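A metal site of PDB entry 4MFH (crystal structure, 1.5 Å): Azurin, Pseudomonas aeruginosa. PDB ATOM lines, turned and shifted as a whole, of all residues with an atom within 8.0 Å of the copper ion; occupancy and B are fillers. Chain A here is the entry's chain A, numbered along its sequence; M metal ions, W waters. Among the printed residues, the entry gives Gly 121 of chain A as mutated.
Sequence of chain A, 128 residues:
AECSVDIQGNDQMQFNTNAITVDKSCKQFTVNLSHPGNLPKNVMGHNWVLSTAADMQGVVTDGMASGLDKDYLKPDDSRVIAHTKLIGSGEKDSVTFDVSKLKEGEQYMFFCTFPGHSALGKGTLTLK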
ATOM      1  N   GLY A   9      24.057  29.132  30.415  1.00  0.00           N
ATOM      2  CA  GLY A   9      24.835  28.571  29.328  1.00  0.00           C
ATOM      3  C   GLY A   9      23.855  28.265  28.198  1.00  0.00           C
ATOM      4  O   GLY A   9      22.705  27.928  28.461  1.00  0.00           O
ATOM      5  N   ASN A  10      24.306  28.417  26.960  1.00  0.00           N
ATOM      6  CA  ASN A  10      23.432  28.280  25.835  1.00  0.00           C
ATOM      7  C   ASN A  10      23.990  27.347  24.765  1.00  0.00           C
ATOM      8  O   ASN A  10      24.527  26.361  25.100  1.00  0.00           O
ATOM      9  CB  ASN A  10      23.015  29.638  25.255  1.00  0.00           C
ATOM     10  CG  ASN A  10      24.158  30.417  24.799  1.00  0.00           C
ATOM     11  OD1 ASN A  10      25.239  29.946  24.655  1.00  0.00           O
ATOM     12  ND2 ASN A  10      23.888  31.676  24.510  1.00  0.00           N
ATOM     13  N   GLN A  12      26.291  27.881  22.726  1.00  0.00           N
ATOM     14  CA  GLN A  12      27.731  28.210  22.588  1.00  0.00           C
ATOM     15  C   GLN A  12      28.404  27.762  24.020  1.00  0.00           C
ATOM     16  O   GLN A  12      27.722  27.254  24.938  1.00  0.00           O
ATOM     17  CB  GLN A  12      27.844  29.716  22.223  1.00  0.00           C
ATOM     18  CG  GLN A  12      27.253  30.247  20.844  1.00  0.00           C
ATOM     19  CD  GLN A  12      25.665  30.244  20.552  1.00  0.00           C
ATOM     20  OE1 GLN A  12      24.836  30.854  21.259  1.00  0.00           O
ATOM     21  NE2 GLN A  12      25.291  29.584  19.461  1.00  0.00           N
ATOM     22  N   MET A  13      29.704  27.920  24.225  1.00  0.00           N
ATOM     23  CA  MET A  13      30.407  27.254  25.402  1.00  0.00           C
ATOM     24  C   MET A  13      30.725  28.261  26.549  1.00  0.00           C
ATOM     25  O   MET A  13      30.985  27.845  27.687  1.00  0.00           O
ATOM     26  CB  MET A  13      31.705  26.534  24.920  1.00  0.00           C
ATOM     27  CG  MET A  13      31.483  25.562  23.737  1.00  0.00           C
ATOM     28  SD  MET A  13      33.040  24.635  23.678  1.00  0.00           S
ATOM     29  CE  MET A  13      34.083  25.782  22.740  1.00  0.00           C
ATOM     30  N   GLN A  14      30.538  29.539  26.262  1.00  0.00           N
ATOM     31  CA  GLN A  14      30.690  30.598  27.288  1.00  0.00           C
ATOM     32  C   GLN A  14      29.432  30.832  28.207  1.00  0.00           C
ATOM     33  O   GLN A  14      28.288  30.912  27.788  1.00  0.00           O
ATOM     34  CB  GLN A  14      30.977  31.950  26.662  1.00  0.00           C
ATOM     35  CG  GLN A  14      32.235  32.061  25.820  1.00  0.00           C
ATOM     36  CD  GLN A  14      32.794  33.481  25.797  1.00  0.00           C
ATOM     37  OE1 GLN A  14      32.110  34.449  25.448  1.00  0.00           O
ATOM     38  NE2 GLN A  14      34.051  33.623  26.206  1.00  0.00           N
ATOM     39  N   PHE A  15      29.721  31.002  29.493  1.00  0.00           N
ATOM     40  CA  PHE A  15      28.688  31.426  30.439  1.00  0.00           C
ATOM     41  C   PHE A  15      28.441  32.890  30.192  1.00  0.00           C
ATOM     42  O   PHE A  15      29.241  33.551  29.616  1.00  0.00           O
ATOM     43  CB  PHE A  15      29.150  31.214  31.912  1.00  0.00           C
ATOM     44  CG  PHE A  15      29.269  29.749  32.398  1.00  0.00           C
ATOM     45  CD1 PHE A  15      28.161  28.954  32.608  1.00  0.00           C
ATOM     46  CD2 PHE A  15      30.547  29.156  32.592  1.00  0.00           C
ATOM     47  CE1 PHE A  15      28.272  27.622  33.101  1.00  0.00           C
ATOM     48  CE2 PHE A  15      30.645  27.866  33.082  1.00  0.00           C
ATOM     49  CZ  PHE A  15      29.530  27.122  33.304  1.00  0.00           C
ATOM     50  N   LEU A  33      21.357  28.084  37.608  1.00  0.00           N
ATOM     51  CA  LEU A  33      21.741  27.891  36.221  1.00  0.00           C
ATOM     52  C   LEU A  33      20.600  27.569  35.322  1.00  0.00           C
ATOM     53  O   LEU A  33      19.732  26.807  35.703  1.00  0.00           O
ATOM     54  CB  LEU A  33      22.798  26.758  36.212  1.00  0.00           C
ATOM     55  CG  LEU A  33      23.424  26.458  34.846  1.00  0.00           C
ATOM     56  CD1 LEU A  33      24.356  27.502  34.377  1.00  0.00           C
ATOM     57  CD2 LEU A  33      24.000  25.073  34.834  1.00  0.00           C
ATOM     58  N   HIS A  35      19.449  27.178  30.859  1.00  0.00           N
ATOM     59  CA  HIS A  35      19.940  26.880  29.465  1.00  0.00           C
ATOM     60  C   HIS A  35      18.887  27.361  28.457  1.00  0.00           C
ATOM     61  O   HIS A  35      17.950  26.615  28.170  1.00  0.00           O
ATOM     62  CB  HIS A  35      20.158  25.375  29.360  1.00  0.00           C
ATOM     63  CG  HIS A  35      20.944  24.947  28.140  1.00  0.00           C
ATOM     64  ND1 HIS A  35      20.732  25.461  26.865  1.00  0.00           N
ATOM     65  CD2 HIS A  35      21.953  24.070  28.046  1.00  0.00           C
ATOM     66  CE1 HIS A  35      21.611  24.894  26.040  1.00  0.00           C
ATOM     67  NE2 HIS A  35      22.327  24.013  26.712  1.00  0.00           N
ATOM     68  N   LYS A  41      21.070  18.108  26.477  1.00  0.00           N
ATOM     69  CA  LYS A  41      22.238  18.012  27.343  1.00  0.00           C
ATOM     70  C   LYS A  41      23.285  17.012  26.846  1.00  0.00           C
ATOM     71  O   LYS A  41      24.406  17.184  27.240  1.00  0.00           O
ATOM     72  CB  LYS A  41      21.824  17.628  28.719  1.00  0.00           C
ATOM     73  CG  LYS A  41      21.435  16.226  28.929  1.00  0.00           C
ATOM     74  CD  LYS A  41      20.955  16.023  30.376  1.00  0.00           C
ATOM     75  CE  LYS A  41      20.465  14.608  30.552  1.00  0.00           C
ATOM     76  NZ  LYS A  41      19.901  14.502  31.915  1.00  0.00           N
ATOM     77  N   VAL A  43      24.414  16.800  23.899  1.00  0.00           N
ATOM     78  CA  VAL A  43      25.107  17.489  22.865  1.00  0.00           C
ATOM     79  C   VAL A  43      25.714  18.841  23.286  1.00  0.00           C
ATOM     80  O   VAL A  43      26.697  19.237  22.799  1.00  0.00           O
ATOM     81  CB  VAL A  43      24.103  17.710  21.654  1.00  0.00           C
ATOM     82  CG1 VAL A  43      24.570  18.768  20.677  1.00  0.00           C
ATOM     83  CG2 VAL A  43      23.926  16.393  20.981  1.00  0.00           C
ATOM     84  N   MET A  44      25.031  19.526  24.162  1.00  0.00           N
ATOM     85  CA  MET A  44      25.448  20.849  24.602  1.00  0.00           C
ATOM     86  C   MET A  44      24.994  21.088  26.011  1.00  0.00           C
ATOM     87  O   MET A  44      24.475  22.086  26.340  1.00  0.00           O
ATOM     88  CB  MET A  44      25.034  22.014  23.698  1.00  0.00           C
ATOM     89  CG  MET A  44      25.975  23.242  23.788  1.00  0.00           C
ATOM     90  SD  MET A  44      27.692  23.064  23.265  1.00  0.00           S
ATOM     91  CE  MET A  44      27.434  22.749  21.536  1.00  0.00           C
ATOM     92  N   GLY A  45      25.223  20.101  26.794  1.00  0.00           N
ATOM     93  CA  GLY A  45      25.003  20.148  28.247  1.00  0.00           C
ATOM     94  C   GLY A  45      25.898  21.142  28.933  1.00  0.00           C
ATOM     95  O   GLY A  45      27.021  21.361  28.541  1.00  0.00           O
ATOM     96  N   HIS A  46      25.404  21.790  30.001  1.00  0.00           N
ATOM     97  CA  HIS A  46      26.241  22.620  30.858  1.00  0.00           C
ATOM     98  C   HIS A  46      25.968  22.286  32.316  1.00  0.00           C
ATOM     99  O   HIS A  46      24.810  22.049  32.721  1.00  0.00           O
ATOM    100  CB  HIS A  46      25.972  24.100  30.658  1.00  0.00           C
ATOM    101  CG  HIS A  46      26.130  24.555  29.250  1.00  0.00           C
ATOM    102  ND1 HIS A  46      27.348  24.505  28.612  1.00  0.00           N
ATOM    103  CD2 HIS A  46      25.250  25.103  28.378  1.00  0.00           C
ATOM    104  CE1 HIS A  46      27.210  25.010  27.389  1.00  0.00           C
ATOM    105  NE2 HIS A  46      25.947  25.387  27.253  1.00  0.00           N
ATOM    106  N   ASN A  47      27.032  22.271  33.086  1.00  0.00           N
ATOM    107  CA  ASN A  47      26.900  22.274  34.548  1.00  0.00           C
ATOM    108  C   ASN A  47      27.711  23.480  35.069  1.00  0.00           C
ATOM    109  O   ASN A  47      28.466  24.145  34.319  1.00  0.00           O
ATOM    110  CB  ASN A  47      27.250  20.957  35.185  1.00  0.00           C
ATOM    111  CG  ASN A  47      28.661  20.433  34.853  1.00  0.00           C
ATOM    112  OD1 ASN A  47      29.507  21.164  34.307  1.00  0.00           O
ATOM    113  ND2 ASN A  47      28.892  19.180  35.132  1.00  0.00           N
ATOM    114  N   TRP A  48      27.538  23.772  36.363  1.00  0.00           N
ATOM    115  CA  TRP A  48      28.314  24.821  37.057  1.00  0.00           C
ATOM    116  C   TRP A  48      28.967  24.084  38.211  1.00  0.00           C
ATOM    117  O   TRP A  48      28.311  23.532  39.060  1.00  0.00           O
ATOM    118  CB  TRP A  48      27.358  25.887  37.518  1.00  0.00           C
ATOM    119  CG  TRP A  48      28.083  27.024  38.214  1.00  0.00           C
ATOM    120  CD1 TRP A  48      28.559  28.174  37.606  1.00  0.00           C
ATOM    121  CD2 TRP A  48      28.472  27.157  39.644  1.00  0.00           C
ATOM    122  NE1 TRP A  48      29.177  28.999  38.547  1.00  0.00           N
ATOM    123  CE2 TRP A  48      29.137  28.394  39.778  1.00  0.00           C
ATOM    124  CE3 TRP A  48      28.294  26.352  40.769  1.00  0.00           C
ATOM    125  CZ2 TRP A  48      29.603  28.824  41.013  1.00  0.00           C
ATOM    126  CZ3 TRP A  48      28.773  26.781  42.000  1.00  0.00           C
ATOM    127  CH2 TRP A  48      29.435  27.987  42.083  1.00  0.00           C
ATOM    128  N   LEU A  86      24.038  18.693  35.307  1.00  0.00           N
ATOM    129  CA  LEU A  86      24.223  18.989  33.911  1.00  0.00           C
ATOM    130  C   LEU A  86      22.824  19.151  33.268  1.00  0.00           C
ATOM    131  O   LEU A  86      21.972  18.295  33.512  1.00  0.00           O
ATOM    132  CB  LEU A  86      24.972  17.801  33.245  1.00  0.00           C
ATOM    133  CG  LEU A  86      25.325  18.064  31.780  1.00  0.00           C
ATOM    134  CD1 LEU A  86      26.615  18.777  31.673  1.00  0.00           C
ATOM    135  CD2 LEU A  86      25.445  16.773  30.951  1.00  0.00           C
ATOM    136  N   ILE A  87      22.628  20.267  32.606  1.00  0.00           N
ATOM    137  CA  ILE A  87      21.331  20.632  32.071  1.00  0.00           C
ATOM    138  C   ILE A  87      21.458  20.881  30.571  1.00  0.00           C
ATOM    139  O   ILE A  87      22.505  21.313  30.064  1.00  0.00           O
ATOM    140  CB  ILE A  87      20.701  21.870  32.773  1.00  0.00           C
ATOM    141  CG1 ILE A  87      21.556  23.115  32.577  1.00  0.00           C
ATOM    142  CG2 ILE A  87      20.518  21.539  34.258  1.00  0.00           C
ATOM    143  CD1 ILE A  87      20.824  24.364  33.109  1.00  0.00           C
ATOM    144  N   PHE A 111      33.340  26.359  36.498  1.00  0.00           N
ATOM    145  CA  PHE A 111      33.546  25.810  35.188  1.00  0.00           C
ATOM    146  C   PHE A 111      32.475  24.746  34.891  1.00  0.00           C
ATOM    147  O   PHE A 111      31.832  24.216  35.726  1.00  0.00           O
ATOM    148  CB  PHE A 111      34.967  25.253  35.041  1.00  0.00           C
ATOM    149  CG  PHE A 111      35.351  24.351  36.112  1.00  0.00           C
ATOM    150  CD1 PHE A 111      35.905  24.827  37.308  1.00  0.00           C
ATOM    151  CD2 PHE A 111      35.107  22.975  36.038  1.00  0.00           C
ATOM    152  CE1 PHE A 111      36.231  23.990  38.341  1.00  0.00           C
ATOM    153  CE2 PHE A 111      35.394  22.158  37.109  1.00  0.00           C
ATOM    154  CZ  PHE A 111      35.997  22.648  38.242  1.00  0.00           C
ATOM    155  N   CYS A 112      32.372  24.445  33.570  1.00  0.00           N
ATOM    156  CA  CYS A 112      31.534  23.392  33.013  1.00  0.00           C
ATOM    157  C   CYS A 112      32.498  22.218  32.707  1.00  0.00           C
ATOM    158  O   CYS A 112      33.552  22.434  32.140  1.00  0.00           O
ATOM    159  CB  CYS A 112      30.821  23.910  31.749  1.00  0.00           C
ATOM    160  SG  CYS A 112      29.826  22.579  31.024  1.00  0.00           S
ATOM    161  N   THR A 113      32.064  21.034  33.050  1.00  0.00           N
ATOM    162  CA  THR A 113      32.835  19.783  32.814  1.00  0.00           C
ATOM    163  C   THR A 113      32.324  19.027  31.548  1.00  0.00           C
ATOM    164  O   THR A 113      32.913  17.924  31.305  1.00  0.00           O
ATOM    165  CB  THR A 113      32.934  18.837  34.011  1.00  0.00           C
ATOM    166  OG1 THR A 113      31.608  18.381  34.338  1.00  0.00           O
ATOM    167  CG2 THR A 113      33.535  19.547  35.174  1.00  0.00           C
ATOM    168  N   PHE A 114      31.292  19.484  30.859  1.00  0.00           N
ATOM    169  CA  PHE A 114      31.020  18.875  29.554  1.00  0.00           C
ATOM    170  C   PHE A 114      32.249  18.870  28.697  1.00  0.00           C
ATOM    171  O   PHE A 114      32.977  19.849  28.671  1.00  0.00           O
ATOM    172  CB  PHE A 114      29.883  19.591  28.932  1.00  0.00           C
ATOM    173  CG  PHE A 114      29.304  18.872  27.746  1.00  0.00           C
ATOM    174  CD1 PHE A 114      29.899  19.027  26.497  1.00  0.00           C
ATOM    175  CD2 PHE A 114      28.198  18.053  27.854  1.00  0.00           C
ATOM    176  CE1 PHE A 114      29.318  18.335  25.392  1.00  0.00           C
ATOM    177  CE2 PHE A 114      27.683  17.378  26.718  1.00  0.00           C
ATOM    178  CZ  PHE A 114      28.175  17.578  25.530  1.00  0.00           C
ATOM    179  N   PRO A 115      32.500  17.793  27.949  1.00  0.00           N
ATOM    180  CA  PRO A 115      33.786  17.735  27.244  1.00  0.00           C
ATOM    181  C   PRO A 115      34.088  18.959  26.386  1.00  0.00           C
ATOM    182  O   PRO A 115      33.326  19.343  25.484  1.00  0.00           O
ATOM    183  CB  PRO A 115      33.586  16.488  26.405  1.00  0.00           C
ATOM    184  CG  PRO A 115      32.797  15.568  27.307  1.00  0.00           C
ATOM    185  CD  PRO A 115      31.778  16.518  27.906  1.00  0.00           C
ATOM    186  N   GLY A 116      35.296  19.497  26.597  1.00  0.00           N
ATOM    187  CA  GLY A 116      35.819  20.645  25.899  1.00  0.00           C
ATOM    188  C   GLY A 116      35.388  22.006  26.367  1.00  0.00           C
ATOM    189  O   GLY A 116      35.864  23.015  25.872  1.00  0.00           O
ATOM    190  N   HIS A 117      34.320  22.052  27.156  1.00  0.00           N
ATOM    191  CA  HIS A 117      33.696  23.332  27.476  1.00  0.00           C
ATOM    192  C   HIS A 117      34.526  24.224  28.392  1.00  0.00           C
ATOM    193  O   HIS A 117      34.291  25.456  28.372  1.00  0.00           O
ATOM    194  CB  HIS A 117      32.311  23.094  28.134  1.00  0.00           C
ATOM    195  CG  HIS A 117      31.248  22.720  27.112  1.00  0.00           C
ATOM    196  ND1 HIS A 117      29.865  22.777  27.282  1.00  0.00           N
ATOM    197  CD2 HIS A 117      31.419  22.226  25.868  1.00  0.00           C
ATOM    198  CE1 HIS A 117      29.270  22.285  26.222  1.00  0.00           C
ATOM    199  NE2 HIS A 117      30.179  21.989  25.345  1.00  0.00           N
ATOM    200  N   SER A 118      35.409  23.652  29.161  1.00  0.00           N
ATOM    201  CA  SER A 118      36.113  24.487  30.162  1.00  0.00           C
ATOM    202  C   SER A 118      37.047  25.497  29.588  1.00  0.00           C
ATOM    203  O   SER A 118      37.358  26.416  30.277  1.00  0.00           O
ATOM    204  CB  SER A 118      36.784  23.609  31.223  1.00  0.00           C
ATOM    205  OG  SER A 118      37.845  22.962  30.674  1.00  0.00           O
ATOM    206  N   GLY A 121      34.264  28.038  29.045  1.00  0.00           N
ATOM    207  CA  GLY A 121      33.164  28.045  30.031  1.00  0.00           C
ATOM    208  C   GLY A 121      33.777  27.902  31.400  1.00  0.00           C
ATOM    209  O   GLY A 121      33.744  26.822  32.030  1.00  0.00           O
HETATM  210 CU    CU M   1      29.095  23.315  29.127  1.00  0.00          CU
HETATM  211  O   HOH W   1      30.128  26.054  29.220  1.00  0.00           O
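Residues that only touch the copper ion: Gly 45 and Phe 114. Of the 26 residues printed, 5 come within 4 Å of the copper ion. The nearest printed residue that does not touch the copper ion is Asn 47 (4.6 Å).
The copper ion is bound by ND1 of His 117. SG of Cys 112 is bound to the copper ion, at 2.2 Å. ND1 of His 46 is bound to the copper ion. The copper ion has three donor atoms within binding distance.
The side-chain sulfur (SD) of Met 44 lies within hydrogen-bond range of a ring nitrogen (NE2) of His 117, at 3.4 Å. O of His 46 lies within hydrogen-bond range of N of Ile 87, 2.8 Å away. SG of Cys 112 lies close to N of Phe 114 (3.4 Å). A ring nitrogen (NE2) of His 46 is in hydrogen-bond range of the backbone carbonyl oxygen (O) of Asn 10 (2.8 Å). The backbone NH (N) of Asn 47 sits close to the side-chain sulfur (SG) of Cys 112, at 3.5 Å. ND1 of His 117 sits close to O of Gly 45, at 3.4 Å. The backbone NH (N) of Cys 112 lies within hydrogen-bond range of the backbone carbonyl oxygen (O) of Gly 121, 3.1 Å away. The backbone carbonyl oxygen (O) of Gln 12 lies close to a ring nitrogen (NE2) of His 46 (3.5 Å).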
